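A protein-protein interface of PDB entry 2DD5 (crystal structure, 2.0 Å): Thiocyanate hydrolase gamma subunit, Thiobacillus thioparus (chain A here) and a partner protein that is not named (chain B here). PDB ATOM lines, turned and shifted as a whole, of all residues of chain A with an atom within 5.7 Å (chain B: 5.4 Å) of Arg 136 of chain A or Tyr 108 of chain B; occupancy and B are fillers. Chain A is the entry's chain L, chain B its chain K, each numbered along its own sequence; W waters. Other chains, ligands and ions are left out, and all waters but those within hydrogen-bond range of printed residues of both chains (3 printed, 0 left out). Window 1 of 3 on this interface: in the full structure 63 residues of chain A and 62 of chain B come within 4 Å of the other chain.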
ATOM      1  N   TYR A  55       2.563 -30.903 -12.834  1.00  0.00           N
ATOM      2  CA  TYR A  55       1.990 -29.925 -11.916  1.00  0.00           C
ATOM      3  C   TYR A  55       2.330 -28.521 -12.406  1.00  0.00           C
ATOM      4  O   TYR A  55       1.451 -27.664 -12.523  1.00  0.00           O
ATOM      5  CB  TYR A  55       2.534 -30.130 -10.498  1.00  0.00           C
ATOM      6  CG  TYR A  55       2.088 -29.061  -9.518  1.00  0.00           C
ATOM      7  CD1 TYR A  55       0.732 -28.817  -9.288  1.00  0.00           C
ATOM      8  CD2 TYR A  55       3.023 -28.266  -8.849  1.00  0.00           C
ATOM      9  CE1 TYR A  55       0.315 -27.801  -8.416  1.00  0.00           C
ATOM     10  CE2 TYR A  55       2.618 -27.253  -7.978  1.00  0.00           C
ATOM     11  CZ  TYR A  55       1.266 -27.024  -7.768  1.00  0.00           C
ATOM     12  OH  TYR A  55       0.871 -26.002  -6.928  1.00  0.00           O
ATOM     13  N   LEU A  59       0.008 -24.853 -13.810  1.00  0.00           N
ATOM     14  CA  LEU A  59       0.080 -23.523 -13.209  1.00  0.00           C
ATOM     15  C   LEU A  59      -0.064 -22.377 -14.207  1.00  0.00           C
ATOM     16  O   LEU A  59       0.171 -22.539 -15.402  1.00  0.00           O
ATOM     17  CB  LEU A  59       1.393 -23.367 -12.430  1.00  0.00           C
ATOM     18  CG  LEU A  59       1.655 -24.432 -11.360  1.00  0.00           C
ATOM     19  CD1 LEU A  59       2.931 -24.084 -10.588  1.00  0.00           C
ATOM     20  CD2 LEU A  59       0.462 -24.520 -10.410  1.00  0.00           C
ATOM     21  N   GLY A  60      -0.448 -21.213 -13.692  1.00  0.00           N
ATOM     22  CA  GLY A  60      -0.637 -20.046 -14.531  1.00  0.00           C
ATOM     23  C   GLY A  60      -1.304 -18.935 -13.740  1.00  0.00           C
ATOM     24  O   GLY A  60      -1.644 -19.129 -12.574  1.00  0.00           O
ATOM     25  N   TRP A  96      -2.977 -24.601  -1.359  1.00  0.00           N
ATOM     26  CA  TRP A  96      -1.539 -24.488  -1.167  1.00  0.00           C
ATOM     27  C   TRP A  96      -0.880 -25.675  -0.481  1.00  0.00           C
ATOM     28  O   TRP A  96       0.322 -25.896  -0.639  1.00  0.00           O
ATOM     29  CB  TRP A  96      -1.212 -23.185  -0.423  1.00  0.00           C
ATOM     30  CG  TRP A  96      -1.410 -21.983  -1.304  1.00  0.00           C
ATOM     31  CD1 TRP A  96      -2.587 -21.556  -1.857  1.00  0.00           C
ATOM     32  CD2 TRP A  96      -0.388 -21.119  -1.819  1.00  0.00           C
ATOM     33  NE1 TRP A  96      -2.359 -20.488  -2.692  1.00  0.00           N
ATOM     34  CE2 TRP A  96      -1.018 -20.198  -2.687  1.00  0.00           C
ATOM     35  CE3 TRP A  96       1.000 -21.036  -1.632  1.00  0.00           C
ATOM     36  CZ2 TRP A  96      -0.306 -19.204  -3.371  1.00  0.00           C
ATOM     37  CZ3 TRP A  96       1.707 -20.047  -2.311  1.00  0.00           C
ATOM     38  CH2 TRP A  96       1.051 -19.145  -3.171  1.00  0.00           C
ATOM     39  N   SER A 108       9.442 -24.838  -2.305  1.00  0.00           N
ATOM     40  CA  SER A 108       9.918 -23.468  -2.482  1.00  0.00           C
ATOM     41  C   SER A 108       8.932 -22.320  -2.287  1.00  0.00           C
ATOM     42  O   SER A 108       9.352 -21.209  -1.964  1.00  0.00           O
ATOM     43  CB  SER A 108      10.564 -23.323  -3.865  1.00  0.00           C
ATOM     44  OG  SER A 108      11.710 -24.152  -3.976  1.00  0.00           O
ATOM     45  N   ASP A 109       7.639 -22.571  -2.476  1.00  0.00           N
ATOM     46  CA  ASP A 109       6.638 -21.512  -2.336  1.00  0.00           C
ATOM     47  C   ASP A 109       5.940 -21.509  -0.977  1.00  0.00           C
ATOM     48  O   ASP A 109       5.321 -20.512  -0.590  1.00  0.00           O
ATOM     49  CB  ASP A 109       5.595 -21.632  -3.452  1.00  0.00           C
ATOM     50  CG  ASP A 109       6.229 -21.796  -4.826  1.00  0.00           C
ATOM     51  OD1 ASP A 109       7.002 -20.902  -5.240  1.00  0.00           O
ATOM     52  OD2 ASP A 109       5.961 -22.826  -5.490  1.00  0.00           O
ATOM     53  N   CSD A 131      15.922 -13.177  -4.131  1.00  0.00           N
ATOM     54  CA  CSD A 131      15.873 -14.141  -5.229  1.00  0.00           C
ATOM     55  CB  CSD A 131      16.078 -15.597  -4.771  1.00  0.00           C
ATOM     56  SG  CSD A 131      15.100 -16.060  -3.286  1.00  0.00           S
ATOM     57  C   CSD A 131      14.860 -13.997  -6.366  1.00  0.00           C
ATOM     58  O   CSD A 131      15.090 -13.282  -7.346  1.00  0.00           O
ATOM     59  N   SER A 132      13.745 -14.696  -6.222  1.00  0.00           N
ATOM     60  CA  SER A 132      12.671 -14.704  -7.204  1.00  0.00           C
ATOM     61  C   SER A 132      11.376 -15.245  -6.590  1.00  0.00           C
ATOM     62  O   SER A 132      10.432 -15.598  -7.294  1.00  0.00           O
ATOM     63  CB  SER A 132      13.073 -15.568  -8.403  1.00  0.00           C
ATOM     64  OG  SER A 132      13.522 -16.849  -7.990  1.00  0.00           O
ATOM     65  N   TYR A 134       8.028 -16.197  -5.575  1.00  0.00           N
ATOM     66  CA  TYR A 134       6.794 -15.887  -6.297  1.00  0.00           C
ATOM     67  C   TYR A 134       5.698 -16.878  -5.889  1.00  0.00           C
ATOM     68  O   TYR A 134       5.990 -18.035  -5.597  1.00  0.00           O
ATOM     69  CB  TYR A 134       7.132 -16.060  -7.776  1.00  0.00           C
ATOM     70  CG  TYR A 134       6.217 -15.455  -8.811  1.00  0.00           C
ATOM     71  CD1 TYR A 134       6.297 -14.104  -9.135  1.00  0.00           C
ATOM     72  CD2 TYR A 134       5.370 -16.264  -9.565  1.00  0.00           C
ATOM     73  CE1 TYR A 134       5.566 -13.577 -10.200  1.00  0.00           C
ATOM     74  CE2 TYR A 134       4.635 -15.752 -10.627  1.00  0.00           C
ATOM     75  CZ  TYR A 134       4.741 -14.414 -10.944  1.00  0.00           C
ATOM     76  OH  TYR A 134       4.053 -13.930 -12.028  1.00  0.00           O
ATOM     77  N   PRO A 135       4.422 -16.443  -5.882  1.00  0.00           N
ATOM     78  CA  PRO A 135       3.313 -17.332  -5.502  1.00  0.00           C
ATOM     79  C   PRO A 135       2.943 -18.303  -6.633  1.00  0.00           C
ATOM     80  O   PRO A 135       1.818 -18.295  -7.140  1.00  0.00           O
ATOM     81  CB  PRO A 135       2.186 -16.352  -5.190  1.00  0.00           C
ATOM     82  CG  PRO A 135       2.421 -15.268  -6.199  1.00  0.00           C
ATOM     83  CD  PRO A 135       3.932 -15.077  -6.155  1.00  0.00           C
ATOM     84  N   ARG A 136       3.899 -19.149  -7.006  1.00  0.00           N
ATOM     85  CA  ARG A 136       3.709 -20.100  -8.097  1.00  0.00           C
ATOM     86  C   ARG A 136       2.413 -20.917  -8.110  1.00  0.00           C
ATOM     87  O   ARG A 136       1.757 -21.013  -9.142  1.00  0.00           O
ATOM     88  CB  ARG A 136       4.902 -21.066  -8.178  1.00  0.00           C
ATOM     89  CG  ARG A 136       6.254 -20.411  -8.484  1.00  0.00           C
ATOM     90  CD  ARG A 136       7.298 -21.498  -8.773  1.00  0.00           C
ATOM     91  NE  ARG A 136       8.627 -20.977  -9.086  1.00  0.00           N
ATOM     92  CZ  ARG A 136       9.588 -20.764  -8.193  1.00  0.00           C
ATOM     93  NH1 ARG A 136       9.384 -21.022  -6.905  1.00  0.00           N
ATOM     94  NH2 ARG A 136      10.765 -20.309  -8.595  1.00  0.00           N
ATOM     95  N   PRO A 137       2.024 -21.519  -6.975  1.00  0.00           N
ATOM     96  CA  PRO A 137       0.787 -22.315  -6.982  1.00  0.00           C
ATOM     97  C   PRO A 137      -0.442 -21.615  -7.561  1.00  0.00           C
ATOM     98  O   PRO A 137      -1.250 -22.233  -8.260  1.00  0.00           O
ATOM     99  CB  PRO A 137       0.607 -22.681  -5.510  1.00  0.00           C
ATOM    100  CG  PRO A 137       2.029 -22.795  -5.029  1.00  0.00           C
ATOM    101  CD  PRO A 137       2.670 -21.569  -5.650  1.00  0.00           C
ATOM    102  N   ILE A 138      -0.577 -20.323  -7.290  1.00  0.00           N
ATOM    103  CA  ILE A 138      -1.733 -19.587  -7.780  1.00  0.00           C
ATOM    104  C   ILE A 138      -1.446 -18.638  -8.946  1.00  0.00           C
ATOM    105  O   ILE A 138      -2.366 -18.222  -9.654  1.00  0.00           O
ATOM    106  CB  ILE A 138      -2.385 -18.786  -6.613  1.00  0.00           C
ATOM    107  CG1 ILE A 138      -3.830 -18.413  -6.962  1.00  0.00           C
ATOM    108  CG2 ILE A 138      -1.579 -17.521  -6.327  1.00  0.00           C
ATOM    109  CD1 ILE A 138      -4.548 -17.691  -5.835  1.00  0.00           C
ATOM    110  N   LEU A 139      -0.176 -18.318  -9.177  1.00  0.00           N
ATOM    111  CA  LEU A 139       0.158 -17.366 -10.234  1.00  0.00           C
ATOM    112  C   LEU A 139       0.979 -17.901 -11.400  1.00  0.00           C
ATOM    113  O   LEU A 139       1.033 -17.276 -12.456  1.00  0.00           O
ATOM    114  CB  LEU A 139       0.871 -16.156  -9.611  1.00  0.00           C
ATOM    115  CG  LEU A 139       1.145 -14.919 -10.476  1.00  0.00           C
ATOM    116  CD1 LEU A 139      -0.163 -14.400 -11.064  1.00  0.00           C
ATOM    117  CD2 LEU A 139       1.803 -13.837  -9.620  1.00  0.00           C
ATOM    118  N   GLY A 140       1.620 -19.051 -11.220  1.00  0.00           N
ATOM    119  CA  GLY A 140       2.424 -19.594 -12.299  1.00  0.00           C
ATOM    120  C   GLY A 140       3.899 -19.263 -12.142  1.00  0.00           C
ATOM    121  O   GLY A 140       4.360 -18.983 -11.039  1.00  0.00           O
ATOM    122  N   GLN A 141       4.641 -19.275 -13.245  1.00  0.00           N
ATOM    123  CA  GLN A 141       6.078 -18.993 -13.199  1.00  0.00           C
ATOM    124  C   GLN A 141       6.405 -17.501 -13.216  1.00  0.00           C
ATOM    125  O   GLN A 141       5.705 -16.713 -13.848  1.00  0.00           O
ATOM    126  CB  GLN A 141       6.776 -19.683 -14.369  1.00  0.00           C
ATOM    127  CG  GLN A 141       6.489 -21.173 -14.440  1.00  0.00           C
ATOM    128  CD  GLN A 141       7.712 -21.976 -14.823  1.00  0.00           C
ATOM    129  OE1 GLN A 141       7.720 -22.678 -15.840  1.00  0.00           O
ATOM    130  NE2 GLN A 141       8.753 -21.884 -14.002  1.00  0.00           N
ATOM    131  N   SER A 142       7.480 -17.126 -12.529  1.00  0.00           N
ATOM    132  CA  SER A 142       7.894 -15.727 -12.461  1.00  0.00           C
ATOM    133  C   SER A 142       8.458 -15.213 -13.784  1.00  0.00           C
ATOM    134  O   SER A 142       9.062 -15.965 -14.551  1.00  0.00           O
ATOM    135  CB  SER A 142       8.943 -15.538 -11.360  1.00  0.00           C
ATOM    136  OG  SER A 142      10.102 -16.318 -11.614  1.00  0.00           O
ATOM    137  N   GLU A 144      10.923 -13.343 -16.432  1.00  0.00           N
ATOM    138  CA  GLU A 144      12.385 -13.288 -16.477  1.00  0.00           C
ATOM    139  C   GLU A 144      12.888 -12.011 -15.777  1.00  0.00           C
ATOM    140  O   GLU A 144      13.838 -12.054 -14.988  1.00  0.00           O
ATOM    141  CB  GLU A 144      12.866 -13.308 -17.938  1.00  0.00           C
ATOM    142  CG  GLU A 144      14.398 -13.265 -18.135  1.00  0.00           C
ATOM    143  CD  GLU A 144      15.106 -14.568 -17.756  1.00  0.00           C
ATOM    144  OE1 GLU A 144      14.429 -15.516 -17.305  1.00  0.00           O
ATOM    145  OE2 GLU A 144      16.349 -14.643 -17.914  1.00  0.00           O
ATOM    146  N   ARG A 147      13.133 -11.836 -11.900  1.00  0.00           N
ATOM    147  CA  ARG A 147      14.286 -12.537 -11.328  1.00  0.00           C
ATOM    148  C   ARG A 147      15.577 -11.744 -11.517  1.00  0.00           C
ATOM    149  O   ARG A 147      16.618 -12.103 -10.958  1.00  0.00           O
ATOM    150  CB  ARG A 147      14.481 -13.885 -12.028  1.00  0.00           C
ATOM    151  CG  ARG A 147      13.234 -14.735 -12.153  1.00  0.00           C
ATOM    152  CD  ARG A 147      13.465 -15.888 -13.138  1.00  0.00           C
ATOM    153  NE  ARG A 147      12.234 -16.638 -13.379  1.00  0.00           N
ATOM    154  CZ  ARG A 147      12.123 -17.656 -14.228  1.00  0.00           C
ATOM    155  NH1 ARG A 147      13.173 -18.062 -14.931  1.00  0.00           N
ATOM    156  NH2 ARG A 147      10.953 -18.261 -14.383  1.00  0.00           N
ATOM    157  N   ARG A 186       4.161 -15.488   0.423  1.00  0.00           N
ATOM    158  CA  ARG A 186       4.137 -15.144  -0.994  1.00  0.00           C
ATOM    159  C   ARG A 186       2.933 -14.210  -1.145  1.00  0.00           C
ATOM    160  O   ARG A 186       1.935 -14.362  -0.439  1.00  0.00           O
ATOM    161  CB  ARG A 186       3.964 -16.393  -1.870  1.00  0.00           C
ATOM    162  CG  ARG A 186       5.123 -17.392  -1.766  1.00  0.00           C
ATOM    163  CD  ARG A 186       6.434 -16.800  -2.303  1.00  0.00           C
ATOM    164  NE  ARG A 186       7.565 -17.709  -2.102  1.00  0.00           N
ATOM    165  CZ  ARG A 186       8.343 -17.725  -1.022  1.00  0.00           C
ATOM    166  NH1 ARG A 186       8.132 -16.872  -0.026  1.00  0.00           N
ATOM    167  NH2 ARG A 186       9.332 -18.610  -0.929  1.00  0.00           N
ATOM    168  N   PHE B  73      14.347 -27.194 -12.619  1.00  0.00           N
ATOM    169  CA  PHE B  73      13.424 -26.758 -11.573  1.00  0.00           C
ATOM    170  C   PHE B  73      12.741 -27.967 -10.932  1.00  0.00           C
ATOM    171  O   PHE B  73      12.686 -28.081  -9.707  1.00  0.00           O
ATOM    172  CB  PHE B  73      12.368 -25.809 -12.151  1.00  0.00           C
ATOM    173  CG  PHE B  73      11.372 -25.322 -11.131  1.00  0.00           C
ATOM    174  CD1 PHE B  73      11.773 -24.488 -10.093  1.00  0.00           C
ATOM    175  CD2 PHE B  73      10.040 -25.710 -11.202  1.00  0.00           C
ATOM    176  CE1 PHE B  73      10.859 -24.046  -9.133  1.00  0.00           C
ATOM    177  CE2 PHE B  73       9.114 -25.276 -10.250  1.00  0.00           C
ATOM    178  CZ  PHE B  73       9.523 -24.442  -9.214  1.00  0.00           C
ATOM    179  N   GLN B  94      22.724 -22.081  -3.302  1.00  0.00           N
ATOM    180  CA  GLN B  94      22.516 -21.558  -4.644  1.00  0.00           C
ATOM    181  C   GLN B  94      22.703 -20.059  -4.867  1.00  0.00           C
ATOM    182  O   GLN B  94      23.289 -19.639  -5.874  1.00  0.00           O
ATOM    183  CB  GLN B  94      21.111 -21.964  -5.083  1.00  0.00           C
ATOM    184  CG  GLN B  94      20.671 -21.462  -6.436  1.00  0.00           C
ATOM    185  CD  GLN B  94      19.175 -21.622  -6.607  1.00  0.00           C
ATOM    186  OE1 GLN B  94      18.657 -22.737  -6.596  1.00  0.00           O
ATOM    187  NE2 GLN B  94      18.470 -20.499  -6.741  1.00  0.00           N
ATOM    188  N   MET B 106      26.994 -16.157 -14.072  1.00  0.00           N
ATOM    189  CA  MET B 106      26.256 -17.265 -14.674  1.00  0.00           C
ATOM    190  C   MET B 106      24.756 -16.996 -14.682  1.00  0.00           C
ATOM    191  O   MET B 106      24.280 -16.111 -13.981  1.00  0.00           O
ATOM    192  CB  MET B 106      26.555 -18.557 -13.913  1.00  0.00           C
ATOM    193  CG  MET B 106      27.956 -19.108 -14.178  1.00  0.00           C
ATOM    194  SD  MET B 106      28.081 -19.853 -15.837  1.00  0.00           S
ATOM    195  CE  MET B 106      27.541 -21.513 -15.454  1.00  0.00           C
ATOM    196  N   PRO B 107      23.996 -17.756 -15.487  1.00  0.00           N
ATOM    197  CA  PRO B 107      22.545 -17.589 -15.579  1.00  0.00           C
ATOM    198  C   PRO B 107      21.824 -18.079 -14.336  1.00  0.00           C
ATOM    199  O   PRO B 107      22.301 -18.972 -13.623  1.00  0.00           O
ATOM    200  CB  PRO B 107      22.160 -18.437 -16.796  1.00  0.00           C
ATOM    201  CG  PRO B 107      23.442 -18.583 -17.567  1.00  0.00           C
ATOM    202  CD  PRO B 107      24.466 -18.734 -16.481  1.00  0.00           C
ATOM    203  N   TYR B 108      20.663 -17.482 -14.104  1.00  0.00           N
ATOM    204  CA  TYR B 108      19.779 -17.817 -12.994  1.00  0.00           C
ATOM    205  C   TYR B 108      19.662 -19.340 -12.832  1.00  0.00           C
ATOM    206  O   TYR B 108      20.073 -19.901 -11.814  1.00  0.00           O
ATOM    207  CB  TYR B 108      18.410 -17.198 -13.299  1.00  0.00           C
ATOM    208  CG  TYR B 108      17.263 -17.576 -12.389  1.00  0.00           C
ATOM    209  CD1 TYR B 108      17.018 -16.879 -11.203  1.00  0.00           C
ATOM    210  CD2 TYR B 108      16.363 -18.573 -12.764  1.00  0.00           C
ATOM    211  CE1 TYR B 108      15.889 -17.162 -10.422  1.00  0.00           C
ATOM    212  CE2 TYR B 108      15.239 -18.867 -11.991  1.00  0.00           C
ATOM    213  CZ  TYR B 108      15.003 -18.160 -10.830  1.00  0.00           C
ATOM    214  OH  TYR B 108      13.864 -18.435 -10.101  1.00  0.00           O
ATOM    215  N   TYR B 109      19.118 -20.014 -13.840  1.00  0.00           N
ATOM    216  CA  TYR B 109      18.951 -21.461 -13.741  1.00  0.00           C
ATOM    217  C   TYR B 109      20.257 -22.250 -13.803  1.00  0.00           C
ATOM    218  O   TYR B 109      20.288 -23.429 -13.457  1.00  0.00           O
ATOM    219  CB  TYR B 109      17.949 -21.956 -14.791  1.00  0.00           C
ATOM    220  CG  TYR B 109      16.525 -22.016 -14.255  1.00  0.00           C
ATOM    221  CD1 TYR B 109      15.468 -21.412 -14.937  1.00  0.00           C
ATOM    222  CD2 TYR B 109      16.236 -22.696 -13.070  1.00  0.00           C
ATOM    223  CE1 TYR B 109      14.156 -21.487 -14.452  1.00  0.00           C
ATOM    224  CE2 TYR B 109      14.928 -22.777 -12.575  1.00  0.00           C
ATOM    225  CZ  TYR B 109      13.898 -22.171 -13.271  1.00  0.00           C
ATOM    226  OH  TYR B 109      12.611 -22.243 -12.784  1.00  0.00           O
ATOM    227  N   GLY B 110      21.337 -21.599 -14.230  1.00  0.00           N
ATOM    228  CA  GLY B 110      22.623 -22.271 -14.258  1.00  0.00           C
ATOM    229  C   GLY B 110      23.035 -22.515 -12.815  1.00  0.00           C
ATOM    230  O   GLY B 110      23.604 -23.554 -12.478  1.00  0.00           O
ATOM    231  N   ARG B 111      22.743 -21.546 -11.952  1.00  0.00           N
ATOM    232  CA  ARG B 111      23.069 -21.674 -10.537  1.00  0.00           C
ATOM    233  C   ARG B 111      22.165 -22.718  -9.880  1.00  0.00           C
ATOM    234  O   ARG B 111      22.609 -23.456  -9.004  1.00  0.00           O
ATOM    235  CB  ARG B 111      22.939 -20.320  -9.828  1.00  0.00           C
ATOM    236  CG  ARG B 111      23.936 -19.282 -10.334  1.00  0.00           C
ATOM    237  CD  ARG B 111      23.865 -17.967  -9.562  1.00  0.00           C
ATOM    238  NE  ARG B 111      22.588 -17.272  -9.743  1.00  0.00           N
ATOM    239  CZ  ARG B 111      21.578 -17.311  -8.879  1.00  0.00           C
ATOM    240  NH1 ARG B 111      21.680 -18.013  -7.759  1.00  0.00           N
ATOM    241  NH2 ARG B 111      20.461 -16.635  -9.133  1.00  0.00           N
ATOM    242  N   TRP B 112      20.899 -22.779 -10.289  1.00  0.00           N
ATOM    243  CA  TRP B 112      19.993 -23.787  -9.731  1.00  0.00           C
ATOM    244  C   TRP B 112      20.553 -25.185 -10.044  1.00  0.00           C
ATOM    245  O   TRP B 112      20.623 -26.051  -9.169  1.00  0.00           O
ATOM    246  CB  TRP B 112      18.587 -23.692 -10.351  1.00  0.00           C
ATOM    247  CG  TRP B 112      17.676 -22.609  -9.809  1.00  0.00           C
ATOM    248  CD1 TRP B 112      17.823 -21.256  -9.953  1.00  0.00           C
ATOM    249  CD2 TRP B 112      16.456 -22.804  -9.071  1.00  0.00           C
ATOM    250  NE1 TRP B 112      16.769 -20.598  -9.353  1.00  0.00           N
ATOM    251  CE2 TRP B 112      15.918 -21.523  -8.807  1.00  0.00           C
ATOM    252  CE3 TRP B 112      15.768 -23.937  -8.611  1.00  0.00           C
ATOM    253  CZ2 TRP B 112      14.717 -21.340  -8.098  1.00  0.00           C
ATOM    254  CZ3 TRP B 112      14.572 -23.757  -7.905  1.00  0.00           C
ATOM    255  CH2 TRP B 112      14.062 -22.464  -7.659  1.00  0.00           C
HETATM  256  O   HOH W   1      11.804 -20.050 -11.250  1.00  0.00           O
HETATM  257  O   HOH W   2      16.211 -18.159  -7.479  1.00  0.00           O
HETATM  258  O   HOH W   3      11.089 -22.470 -14.801  1.00  0.00           O
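Of the 20 printed residues of chain A, 3 touch a printed residue of chain B.
Printed residues of chain B that touch a printed residue of chain A: Phe 73, Tyr 108 and Tyr 109.
Hydrophobic or aromatic side chains of chain B that line the printed part of chain A: Phe 73, Tyr 108 and Tyr 109.
Among the printed residues, no Asp or Glu carboxylate lies within 4 Å of a Lys or Arg side-chain nitrogen of the other chain.
OD1 of Asp 109 of chain A is in salt-bridge range of NH1 of Arg 136 of chain A (2.9 Å).
OG of Ser 142 of chain A lies within hydrogen-bond range of NE of Arg 147 of chain A.
OE1 of Glu 144 of chain A is in salt-bridge range of NH1 of Arg 147 of chain A, 3.7 Å away.
Of chain B, only Phe 73 (3.6 Å) and Tyr 108 (3.9 Å) come within 4 Å of Arg 136 of chain A.
Of the printed residues of chain A, Tyr 109 of chain B touches Arg 147.
Printed residues of chain B within 4 Å of Ser 132 of chain A: Tyr 108 (2.7 Å).
Printed residues of chain B within 4 Å of Arg 147 of chain A: Tyr 108 (3.6 Å) and Tyr 109 (3.6 Å).
Printed residues of chain A within 4 Å of Phe 73 of chain B: Arg 136 (3.6 Å).
Gln 94 of chain B touches none of the printed residues of chain A.
The nearest residue of chain B that does not touch Arg 136 of chain A is Trp 112 of chain B (4.05 Å).
The side-chain hydroxyl (OG) of Ser 132 of chain A lies within hydrogen-bond range of the side-chain hydroxyl (OH) of Tyr 108 of chain B.
Among the printed residues, pairs that only touch across the chains: Arg 136 of chain A with Phe 73 of chain B (3.6 Å), Arg 147 of chain A with Tyr 108 of chain B (3.6 Å), Arg 147 of chain A with Tyr 109 of chain B (3.6 Å) and Arg 136 of chain A with Tyr 108 of chain B (3.9 Å).
Water W3 bridges NE2 of Gln 141 of chain A (2.5 Å) and OH of Tyr 109 of chain B (2.5 Å).
Water W1 lies within hydrogen-bond range of the side-chain hydroxyl (OH) of Tyr 109 of chain B (2.8 Å), the side-chain hydroxyl (OH) of Tyr 108 of chain B (2.9 Å) and the guanidinium group (NH2) of Arg 136 of chain A (2.9 Å).
Water W2 lies within hydrogen-bond range of the side-chain hydroxyl of Ser 132 of chain A (3.0 Å), the indole nitrogen of Trp 112 of chain B (3.1 Å) and the side-chain amide nitrogen of Gln 94 of chain B (3.3 Å).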
